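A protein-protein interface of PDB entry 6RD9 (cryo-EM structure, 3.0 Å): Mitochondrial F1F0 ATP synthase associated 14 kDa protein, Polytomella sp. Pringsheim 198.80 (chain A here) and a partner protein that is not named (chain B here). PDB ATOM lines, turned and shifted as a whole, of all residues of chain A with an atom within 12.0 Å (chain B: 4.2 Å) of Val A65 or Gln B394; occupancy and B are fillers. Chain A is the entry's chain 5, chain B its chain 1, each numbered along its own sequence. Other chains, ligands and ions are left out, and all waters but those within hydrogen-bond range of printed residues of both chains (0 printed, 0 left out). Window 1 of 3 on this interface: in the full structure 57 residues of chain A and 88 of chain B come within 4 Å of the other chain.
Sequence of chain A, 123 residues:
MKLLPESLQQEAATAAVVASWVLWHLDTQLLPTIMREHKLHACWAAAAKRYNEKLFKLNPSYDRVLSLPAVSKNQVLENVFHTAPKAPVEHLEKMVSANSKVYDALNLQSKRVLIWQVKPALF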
ATOM      1  N   ASN A  59     -26.316   5.666  -5.367  1.00  0.00           N
ATOM      2  CA  ASN A  59     -24.976   5.625  -5.923  1.00  0.00           C
ATOM      3  C   ASN A  59     -24.301   6.968  -5.696  1.00  0.00           C
ATOM      4  O   ASN A  59     -24.943   8.008  -5.831  1.00  0.00           O
ATOM      5  CB  ASN A  59     -24.959   5.221  -7.405  1.00  0.00           C
ATOM      6  CG  ASN A  59     -25.450   6.271  -8.310  1.00  0.00           C
ATOM      7  OD1 ASN A  59     -26.400   6.950  -8.005  1.00  0.00           O
ATOM      8  ND2 ASN A  59     -24.800   6.429  -9.436  1.00  0.00           N
ATOM      9  N   PRO A  60     -23.049   6.976  -5.265  1.00  0.00           N
ATOM     10  CA  PRO A  60     -22.435   8.210  -4.786  1.00  0.00           C
ATOM     11  C   PRO A  60     -21.720   8.953  -5.885  1.00  0.00           C
ATOM     12  O   PRO A  60     -20.958   9.882  -5.640  1.00  0.00           O
ATOM     13  CB  PRO A  60     -21.472   7.699  -3.724  1.00  0.00           C
ATOM     14  CG  PRO A  60     -21.078   6.387  -4.228  1.00  0.00           C
ATOM     15  CD  PRO A  60     -22.150   5.830  -5.077  1.00  0.00           C
ATOM     16  N   SER A  61     -22.002   8.553  -7.103  1.00  0.00           N
ATOM     17  CA  SER A  61     -21.240   8.897  -8.279  1.00  0.00           C
ATOM     18  C   SER A  61     -21.485  10.289  -8.814  1.00  0.00           C
ATOM     19  O   SER A  61     -20.906  10.627  -9.842  1.00  0.00           O
ATOM     20  CB  SER A  61     -21.565   7.910  -9.371  1.00  0.00           C
ATOM     21  OG  SER A  61     -21.127   8.426 -10.589  1.00  0.00           O
ATOM     22  N   TYR A  62     -22.311  11.106  -8.186  1.00  0.00           N
ATOM     23  CA  TYR A  62     -22.618  12.401  -8.775  1.00  0.00           C
ATOM     24  C   TYR A  62     -21.869  13.541  -8.129  1.00  0.00           C
ATOM     25  O   TYR A  62     -21.428  14.457  -8.821  1.00  0.00           O
ATOM     26  CB  TYR A  62     -24.103  12.694  -8.672  1.00  0.00           C
ATOM     27  CG  TYR A  62     -24.958  11.631  -9.247  1.00  0.00           C
ATOM     28  CD1 TYR A  62     -24.973  11.404 -10.597  1.00  0.00           C
ATOM     29  CD2 TYR A  62     -25.775  10.884  -8.445  1.00  0.00           C
ATOM     30  CE1 TYR A  62     -25.754  10.450 -11.123  1.00  0.00           C
ATOM     31  CE2 TYR A  62     -26.555   9.928  -8.967  1.00  0.00           C
ATOM     32  CZ  TYR A  62     -26.534   9.710 -10.305  1.00  0.00           C
ATOM     33  OH  TYR A  62     -27.327   8.751 -10.841  1.00  0.00           O
ATOM     34  N   ASP A  63     -21.755  13.518  -6.812  1.00  0.00           N
ATOM     35  CA  ASP A  63     -21.085  14.555  -6.050  1.00  0.00           C
ATOM     36  C   ASP A  63     -19.723  14.095  -5.590  1.00  0.00           C
ATOM     37  O   ASP A  63     -19.355  14.278  -4.433  1.00  0.00           O
ATOM     38  CB  ASP A  63     -21.950  14.971  -4.875  1.00  0.00           C
ATOM     39  CG  ASP A  63     -22.524  13.796  -4.136  1.00  0.00           C
ATOM     40  OD1 ASP A  63     -22.320  12.656  -4.588  1.00  0.00           O
ATOM     41  OD2 ASP A  63     -23.194  14.007  -3.103  1.00  0.00           O
ATOM     42  N   ARG A  64     -18.984  13.431  -6.473  1.00  0.00           N
ATOM     43  CA  ARG A  64     -17.616  13.060  -6.167  1.00  0.00           C
ATOM     44  C   ARG A  64     -16.706  14.264  -6.109  1.00  0.00           C
ATOM     45  O   ARG A  64     -15.671  14.208  -5.444  1.00  0.00           O
ATOM     46  CB  ARG A  64     -17.079  12.095  -7.207  1.00  0.00           C
ATOM     47  CG  ARG A  64     -17.748  10.774  -7.241  1.00  0.00           C
ATOM     48  CD  ARG A  64     -17.280   9.873  -6.139  1.00  0.00           C
ATOM     49  NE  ARG A  64     -17.530   8.497  -6.524  1.00  0.00           N
ATOM     50  CZ  ARG A  64     -17.704   7.497  -5.677  1.00  0.00           C
ATOM     51  NH1 ARG A  64     -17.661   7.707  -4.375  1.00  0.00           N
ATOM     52  NH2 ARG A  64     -17.937   6.288  -6.138  1.00  0.00           N
ATOM     53  N   VAL A  65     -17.075  15.350  -6.788  1.00  0.00           N
ATOM     54  CA  VAL A  65     -16.267  16.552  -6.798  1.00  0.00           C
ATOM     55  C   VAL A  65     -16.270  17.229  -5.441  1.00  0.00           C
ATOM     56  O   VAL A  65     -15.337  17.964  -5.118  1.00  0.00           O
ATOM     57  CB  VAL A  65     -16.764  17.477  -7.923  1.00  0.00           C
ATOM     58  CG1 VAL A  65     -18.058  18.136  -7.559  1.00  0.00           C
ATOM     59  CG2 VAL A  65     -15.724  18.491  -8.291  1.00  0.00           C
ATOM     60  N   LEU A  66     -17.258  16.960  -4.602  1.00  0.00           N
ATOM     61  CA  LEU A  66     -17.282  17.537  -3.276  1.00  0.00           C
ATOM     62  C   LEU A  66     -16.420  16.774  -2.299  1.00  0.00           C
ATOM     63  O   LEU A  66     -16.345  17.163  -1.137  1.00  0.00           O
ATOM     64  CB  LEU A  66     -18.709  17.597  -2.755  1.00  0.00           C
ATOM     65  CG  LEU A  66     -19.761  18.306  -3.584  1.00  0.00           C
ATOM     66  CD1 LEU A  66     -20.968  18.506  -2.744  1.00  0.00           C
ATOM     67  CD2 LEU A  66     -19.265  19.617  -4.061  1.00  0.00           C
ATOM     68  N   SER A  67     -15.788  15.692  -2.720  1.00  0.00           N
ATOM     69  CA  SER A  67     -14.801  15.019  -1.897  1.00  0.00           C
ATOM     70  C   SER A  67     -13.382  15.366  -2.298  1.00  0.00           C
ATOM     71  O   SER A  67     -12.455  15.080  -1.540  1.00  0.00           O
ATOM     72  CB  SER A  67     -14.988  13.506  -1.963  1.00  0.00           C
ATOM     73  OG  SER A  67     -16.287  13.142  -1.542  1.00  0.00           O
ATOM     74  N   LEU A  68     -13.198  15.966  -3.464  1.00  0.00           N
ATOM     75  CA  LEU A  68     -11.913  16.500  -3.854  1.00  0.00           C
ATOM     76  C   LEU A  68     -11.584  17.712  -2.991  1.00  0.00           C
ATOM     77  O   LEU A  68     -12.484  18.343  -2.437  1.00  0.00           O
ATOM     78  CB  LEU A  68     -11.947  16.897  -5.318  1.00  0.00           C
ATOM     79  CG  LEU A  68     -12.068  15.776  -6.326  1.00  0.00           C
ATOM     80  CD1 LEU A  68     -11.901  16.351  -7.692  1.00  0.00           C
ATOM     81  CD2 LEU A  68     -11.055  14.707  -6.076  1.00  0.00           C
ATOM     82  N   PRO A  69     -10.303  18.056  -2.851  1.00  0.00           N
ATOM     83  CA  PRO A  69      -9.949  19.262  -2.099  1.00  0.00           C
ATOM     84  C   PRO A  69     -10.414  20.514  -2.822  1.00  0.00           C
ATOM     85  O   PRO A  69     -10.094  20.723  -3.991  1.00  0.00           O
ATOM     86  CB  PRO A  69      -8.428  19.184  -2.016  1.00  0.00           C
ATOM     87  CG  PRO A  69      -8.044  18.285  -3.088  1.00  0.00           C
ATOM     88  CD  PRO A  69      -9.099  17.280  -3.181  1.00  0.00           C
ATOM     89  N   ALA A  70     -11.193  21.335  -2.111  1.00  0.00           N
ATOM     90  CA  ALA A  70     -11.893  22.451  -2.736  1.00  0.00           C
ATOM     91  C   ALA A  70     -10.944  23.550  -3.138  1.00  0.00           C
ATOM     92  O   ALA A  70     -11.226  24.295  -4.080  1.00  0.00           O
ATOM     93  CB  ALA A  70     -12.946  23.017  -1.798  1.00  0.00           C
ATOM     94  N   VAL A  71      -9.827  23.671  -2.432  1.00  0.00           N
ATOM     95  CA  VAL A  71      -8.813  24.647  -2.785  1.00  0.00           C
ATOM     96  C   VAL A  71      -8.123  24.172  -4.048  1.00  0.00           C
ATOM     97  O   VAL A  71      -7.617  23.050  -4.108  1.00  0.00           O
ATOM     98  CB  VAL A  71      -7.814  24.834  -1.644  1.00  0.00           C
ATOM     99  CG1 VAL A  71      -6.953  26.009  -1.926  1.00  0.00           C
ATOM    100  CG2 VAL A  71      -8.535  25.038  -0.358  1.00  0.00           C
ATOM    101  N   SER A  72      -8.092  25.030  -5.053  1.00  0.00           N
ATOM    102  CA  SER A  72      -7.627  24.670  -6.374  1.00  0.00           C
ATOM    103  C   SER A  72      -6.131  24.413  -6.398  1.00  0.00           C
ATOM    104  O   SER A  72      -5.416  24.663  -5.435  1.00  0.00           O
ATOM    105  CB  SER A  72      -7.949  25.781  -7.349  1.00  0.00           C
ATOM    106  OG  SER A  72      -7.538  25.414  -8.641  1.00  0.00           O
ATOM    107  N   LYS A  73      -5.659  23.886  -7.522  1.00  0.00           N
ATOM    108  CA  LYS A  73      -4.225  23.844  -7.750  1.00  0.00           C
ATOM    109  C   LYS A  73      -3.694  25.230  -8.041  1.00  0.00           C
ATOM    110  O   LYS A  73      -2.547  25.532  -7.721  1.00  0.00           O
ATOM    111  CB  LYS A  73      -3.909  22.893  -8.895  1.00  0.00           C
ATOM    112  CG  LYS A  73      -2.444  22.626  -9.106  1.00  0.00           C
ATOM    113  CD  LYS A  73      -1.776  22.210  -7.820  1.00  0.00           C
ATOM    114  CE  LYS A  73      -0.332  21.851  -8.039  1.00  0.00           C
ATOM    115  NZ  LYS A  73       0.175  21.135  -6.855  1.00  0.00           N
ATOM    116  N   ASN A  74      -4.518  26.074  -8.645  1.00  0.00           N
ATOM    117  CA  ASN A  74      -4.171  27.473  -8.827  1.00  0.00           C
ATOM    118  C   ASN A  74      -3.996  28.183  -7.501  1.00  0.00           C
ATOM    119  O   ASN A  74      -3.022  28.910  -7.314  1.00  0.00           O
ATOM    120  CB  ASN A  74      -5.254  28.169  -9.612  1.00  0.00           C
ATOM    121  CG  ASN A  74      -4.946  29.583  -9.834  1.00  0.00           C
ATOM    122  OD1 ASN A  74      -3.801  29.948 -10.011  1.00  0.00           O
ATOM    123  ND2 ASN A  74      -5.949  30.420  -9.723  1.00  0.00           N
ATOM    124  N   GLN A  75      -4.923  27.998  -6.571  1.00  0.00           N
ATOM    125  CA  GLN A  75      -4.854  28.698  -5.301  1.00  0.00           C
ATOM    126  C   GLN A  75      -3.756  28.174  -4.403  1.00  0.00           C
ATOM    127  O   GLN A  75      -3.434  28.820  -3.411  1.00  0.00           O
ATOM    128  CB  GLN A  75      -6.170  28.584  -4.569  1.00  0.00           C
ATOM    129  CG  GLN A  75      -7.318  29.136  -5.334  1.00  0.00           C
ATOM    130  CD  GLN A  75      -8.541  29.256  -4.491  1.00  0.00           C
ATOM    131  OE1 GLN A  75      -8.596  28.737  -3.392  1.00  0.00           O
ATOM    132  NE2 GLN A  75      -9.525  29.971  -4.987  1.00  0.00           N
ATOM    133  N   PHE B 111     -22.620  22.898  -6.882  1.00  0.00           N
ATOM    134  CA  PHE B 111     -21.322  22.308  -6.593  1.00  0.00           C
ATOM    135  C   PHE B 111     -20.250  23.373  -6.505  1.00  0.00           C
ATOM    136  O   PHE B 111     -19.280  23.221  -5.766  1.00  0.00           O
ATOM    137  CB  PHE B 111     -20.950  21.296  -7.670  1.00  0.00           C
ATOM    138  CG  PHE B 111     -21.659  19.991  -7.556  1.00  0.00           C
ATOM    139  CD1 PHE B 111     -22.164  19.561  -6.351  1.00  0.00           C
ATOM    140  CD2 PHE B 111     -21.806  19.187  -8.659  1.00  0.00           C
ATOM    141  CE1 PHE B 111     -22.809  18.365  -6.258  1.00  0.00           C
ATOM    142  CE2 PHE B 111     -22.449  17.992  -8.562  1.00  0.00           C
ATOM    143  CZ  PHE B 111     -22.947  17.588  -7.359  1.00  0.00           C
ATOM    144  N   ILE B 115     -17.942  24.235  -3.095  1.00  0.00           N
ATOM    145  CA  ILE B 115     -16.493  24.215  -3.213  1.00  0.00           C
ATOM    146  C   ILE B 115     -15.915  25.565  -2.831  1.00  0.00           C
ATOM    147  O   ILE B 115     -15.024  25.652  -1.983  1.00  0.00           O
ATOM    148  CB  ILE B 115     -16.094  23.809  -4.636  1.00  0.00           C
ATOM    149  CG1 ILE B 115     -16.284  22.315  -4.812  1.00  0.00           C
ATOM    150  CG2 ILE B 115     -14.680  24.133  -4.897  1.00  0.00           C
ATOM    151  CD1 ILE B 115     -16.172  21.887  -6.227  1.00  0.00           C
ATOM    152  N   THR B 384      -9.100  21.277 -19.488  1.00  0.00           N
ATOM    153  CA  THR B 384     -10.099  22.052 -18.764  1.00  0.00           C
ATOM    154  C   THR B 384     -11.253  22.452 -19.662  1.00  0.00           C
ATOM    155  O   THR B 384     -12.393  22.530 -19.211  1.00  0.00           O
ATOM    156  CB  THR B 384      -9.441  23.275 -18.149  1.00  0.00           C
ATOM    157  OG1 THR B 384      -8.227  22.866 -17.524  1.00  0.00           O
ATOM    158  CG2 THR B 384     -10.299  23.879 -17.128  1.00  0.00           C
ATOM    159  N   TYR B 388     -14.895  20.648 -18.331  1.00  0.00           N
ATOM    160  CA  TYR B 388     -15.801  21.622 -17.752  1.00  0.00           C
ATOM    161  C   TYR B 388     -16.298  22.566 -18.825  1.00  0.00           C
ATOM    162  O   TYR B 388     -15.644  22.775 -19.842  1.00  0.00           O
ATOM    163  CB  TYR B 388     -15.144  22.443 -16.664  1.00  0.00           C
ATOM    164  CG  TYR B 388     -14.296  21.655 -15.726  1.00  0.00           C
ATOM    165  CD1 TYR B 388     -14.859  20.952 -14.690  1.00  0.00           C
ATOM    166  CD2 TYR B 388     -12.932  21.614 -15.878  1.00  0.00           C
ATOM    167  CE1 TYR B 388     -14.086  20.235 -13.839  1.00  0.00           C
ATOM    168  CE2 TYR B 388     -12.153  20.903 -15.027  1.00  0.00           C
ATOM    169  CZ  TYR B 388     -12.735  20.213 -14.012  1.00  0.00           C
ATOM    170  OH  TYR B 388     -11.948  19.492 -13.160  1.00  0.00           O
ATOM    171  N   ARG B 392     -18.388  26.941 -15.188  1.00  0.00           N
ATOM    172  CA  ARG B 392     -17.992  26.283 -13.959  1.00  0.00           C
ATOM    173  C   ARG B 392     -16.917  27.057 -13.221  1.00  0.00           C
ATOM    174  O   ARG B 392     -16.241  27.913 -13.774  1.00  0.00           O
ATOM    175  CB  ARG B 392     -17.494  24.877 -14.248  1.00  0.00           C
ATOM    176  CG  ARG B 392     -18.480  24.042 -14.981  1.00  0.00           C
ATOM    177  CD  ARG B 392     -19.729  23.844 -14.184  1.00  0.00           C
ATOM    178  NE  ARG B 392     -19.469  23.230 -12.895  1.00  0.00           N
ATOM    179  CZ  ARG B 392     -19.361  21.924 -12.703  1.00  0.00           C
ATOM    180  NH1 ARG B 392     -19.471  21.096 -13.721  1.00  0.00           N
ATOM    181  NH2 ARG B 392     -19.125  21.446 -11.497  1.00  0.00           N
ATOM    182  N   LEU B 393     -16.791  26.748 -11.940  1.00  0.00           N
ATOM    183  CA  LEU B 393     -15.705  27.282 -11.140  1.00  0.00           C
ATOM    184  C   LEU B 393     -14.384  26.683 -11.559  1.00  0.00           C
ATOM    185  O   LEU B 393     -13.371  27.377 -11.619  1.00  0.00           O
ATOM    186  CB  LEU B 393     -15.943  26.970  -9.678  1.00  0.00           C
ATOM    187  CG  LEU B 393     -14.930  27.509  -8.703  1.00  0.00           C
ATOM    188  CD1 LEU B 393     -15.136  28.979  -8.619  1.00  0.00           C
ATOM    189  CD2 LEU B 393     -15.116  26.855  -7.387  1.00  0.00           C
ATOM    190  N   GLN B 394     -14.375  25.390 -11.835  1.00  0.00           N
ATOM    191  CA  GLN B 394     -13.144  24.686 -12.112  1.00  0.00           C
ATOM    192  C   GLN B 394     -12.666  24.888 -13.529  1.00  0.00           C
ATOM    193  O   GLN B 394     -11.542  24.502 -13.840  1.00  0.00           O
ATOM    194  CB  GLN B 394     -13.341  23.216 -11.822  1.00  0.00           C
ATOM    195  CG  GLN B 394     -13.926  23.003 -10.464  1.00  0.00           C
ATOM    196  CD  GLN B 394     -14.013  21.560 -10.091  1.00  0.00           C
ATOM    197  OE1 GLN B 394     -14.633  20.768 -10.786  1.00  0.00           O
ATOM    198  NE2 GLN B 394     -13.385  21.199  -8.985  1.00  0.00           N
ATOM    199  N   TYR B 395     -13.488  25.464 -14.392  1.00  0.00           N
ATOM    200  CA  TYR B 395     -12.977  25.975 -15.648  1.00  0.00           C
ATOM    201  C   TYR B 395     -12.175  27.236 -15.410  1.00  0.00           C
ATOM    202  O   TYR B 395     -11.121  27.436 -16.017  1.00  0.00           O
ATOM    203  CB  TYR B 395     -14.124  26.254 -16.596  1.00  0.00           C
ATOM    204  CG  TYR B 395     -13.740  26.711 -17.972  1.00  0.00           C
ATOM    205  CD1 TYR B 395     -13.547  25.806 -18.979  1.00  0.00           C
ATOM    206  CD2 TYR B 395     -13.615  28.057 -18.275  1.00  0.00           C
ATOM    207  CE1 TYR B 395     -13.219  26.212 -20.231  1.00  0.00           C
ATOM    208  CE2 TYR B 395     -13.289  28.470 -19.529  1.00  0.00           C
ATOM    209  CZ  TYR B 395     -13.095  27.539 -20.503  1.00  0.00           C
ATOM    210  OH  TYR B 395     -12.767  27.935 -21.769  1.00  0.00           O
ATOM    211  N   LYS B 396     -12.676  28.107 -14.544  1.00  0.00           N
ATOM    212  CA  LYS B 396     -11.975  29.341 -14.236  1.00  0.00           C
ATOM    213  C   LYS B 396     -10.702  29.075 -13.452  1.00  0.00           C
ATOM    214  O   LYS B 396      -9.685  29.718 -13.695  1.00  0.00           O
ATOM    215  CB  LYS B 396     -12.901  30.272 -13.476  1.00  0.00           C
ATOM    216  CG  LYS B 396     -14.114  30.645 -14.276  1.00  0.00           C
ATOM    217  CD  LYS B 396     -15.218  31.156 -13.397  1.00  0.00           C
ATOM    218  CE  LYS B 396     -16.440  31.456 -14.218  1.00  0.00           C
ATOM    219  NZ  LYS B 396     -17.583  31.771 -13.340  1.00  0.00           N
ATOM    220  N   GLU B 397     -10.723  28.118 -12.534  1.00  0.00           N
ATOM    221  CA  GLU B 397      -9.514  27.794 -11.797  1.00  0.00           C
ATOM    222  C   GLU B 397      -8.552  26.949 -12.598  1.00  0.00           C
ATOM    223  O   GLU B 397      -7.449  26.680 -12.125  1.00  0.00           O
ATOM    224  CB  GLU B 397      -9.839  27.059 -10.510  1.00  0.00           C
ATOM    225  CG  GLU B 397     -10.645  27.860  -9.544  1.00  0.00           C
ATOM    226  CD  GLU B 397      -9.900  29.057  -9.019  1.00  0.00           C
ATOM    227  OE1 GLU B 397      -8.693  28.942  -8.745  1.00  0.00           O
ATOM    228  OE2 GLU B 397     -10.528  30.124  -8.882  1.00  0.00           O
ATOM    229  N   GLY B 398      -8.953  26.477 -13.761  1.00  0.00           N
ATOM    230  CA  GLY B 398      -8.088  25.628 -14.538  1.00  0.00           C
ATOM    231  C   GLY B 398      -7.381  26.428 -15.591  1.00  0.00           C
ATOM    232  O   GLY B 398      -6.266  26.110 -15.987  1.00  0.00           O
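OE1 of Glu B397 sits at hydrogen-bond distance from ND2 of Asn A74 (3.3 Å).
The side-chain hydroxyl (OG) of Ser A72 sits at hydrogen-bond distance from the backbone NH (N) of Asn A74 (3.1 Å).
The side-chain amide oxygen of Asn A59 lies close to the side-chain hydroxyl of Tyr A62, at 3.5 Å.
Among the printed residues, merely in contact across the chains: Tyr A62 with Phe B111 (3.7 Å), Asp A63 with Phe B111 (3.7 Å), Val A65 with Ile B115 (3.999 Å), Val A65 with Gln B394 (3.5 Å), Leu A66 with Phe B111 (3.7 Å), Ala A70 with Ile B115 (3.4 Å), Ser A72 with Glu B397 (3.4 Å) and Gln A75 with Glu B397 (3.7 Å).
Of chain A, only Val A65 (3.5 Å) comes within 4 Å of Gln B394.
Of chain A, only Tyr A62, Asp A63 and Leu A66 come within 4 Å of Phe B111.
No residue of chain A comes within 4 Å of Thr B384.
No residue of chain A comes within 4 Å of Tyr B388.
No residue of chain A comes within 4 Å of Arg B392.
No residue of chain A comes within 4 Å of Leu B393.
No residue of chain A comes within 4 Å of Lys B396.
No residue of chain A comes within 4 Å of Gly B398.
Printed residues of chain B within 4 Å of Asn A74: Glu B397 (3.3 Å).
Printed residues of chain B within 4 Å of Ser A72: Glu B397 (3.4 Å).
Of the printed residues of chain B, Ala A70 touches Ile B115 (3.4 Å).
Printed residues of chain B within 4 Å of Gln A75: Glu B397 (3.7 Å).
The nearest printed residue of chain B that does not touch Val A65 is Phe B111 (4.05 Å).
Hydrophobic or aromatic side chains of chain A that line the printed part of chain B: Val A65, Leu A66 and Ala A70.
Among the printed residues, no Asp or Glu carboxylate lies within 4 Å of a Lys or Arg side-chain nitrogen of the other chain.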
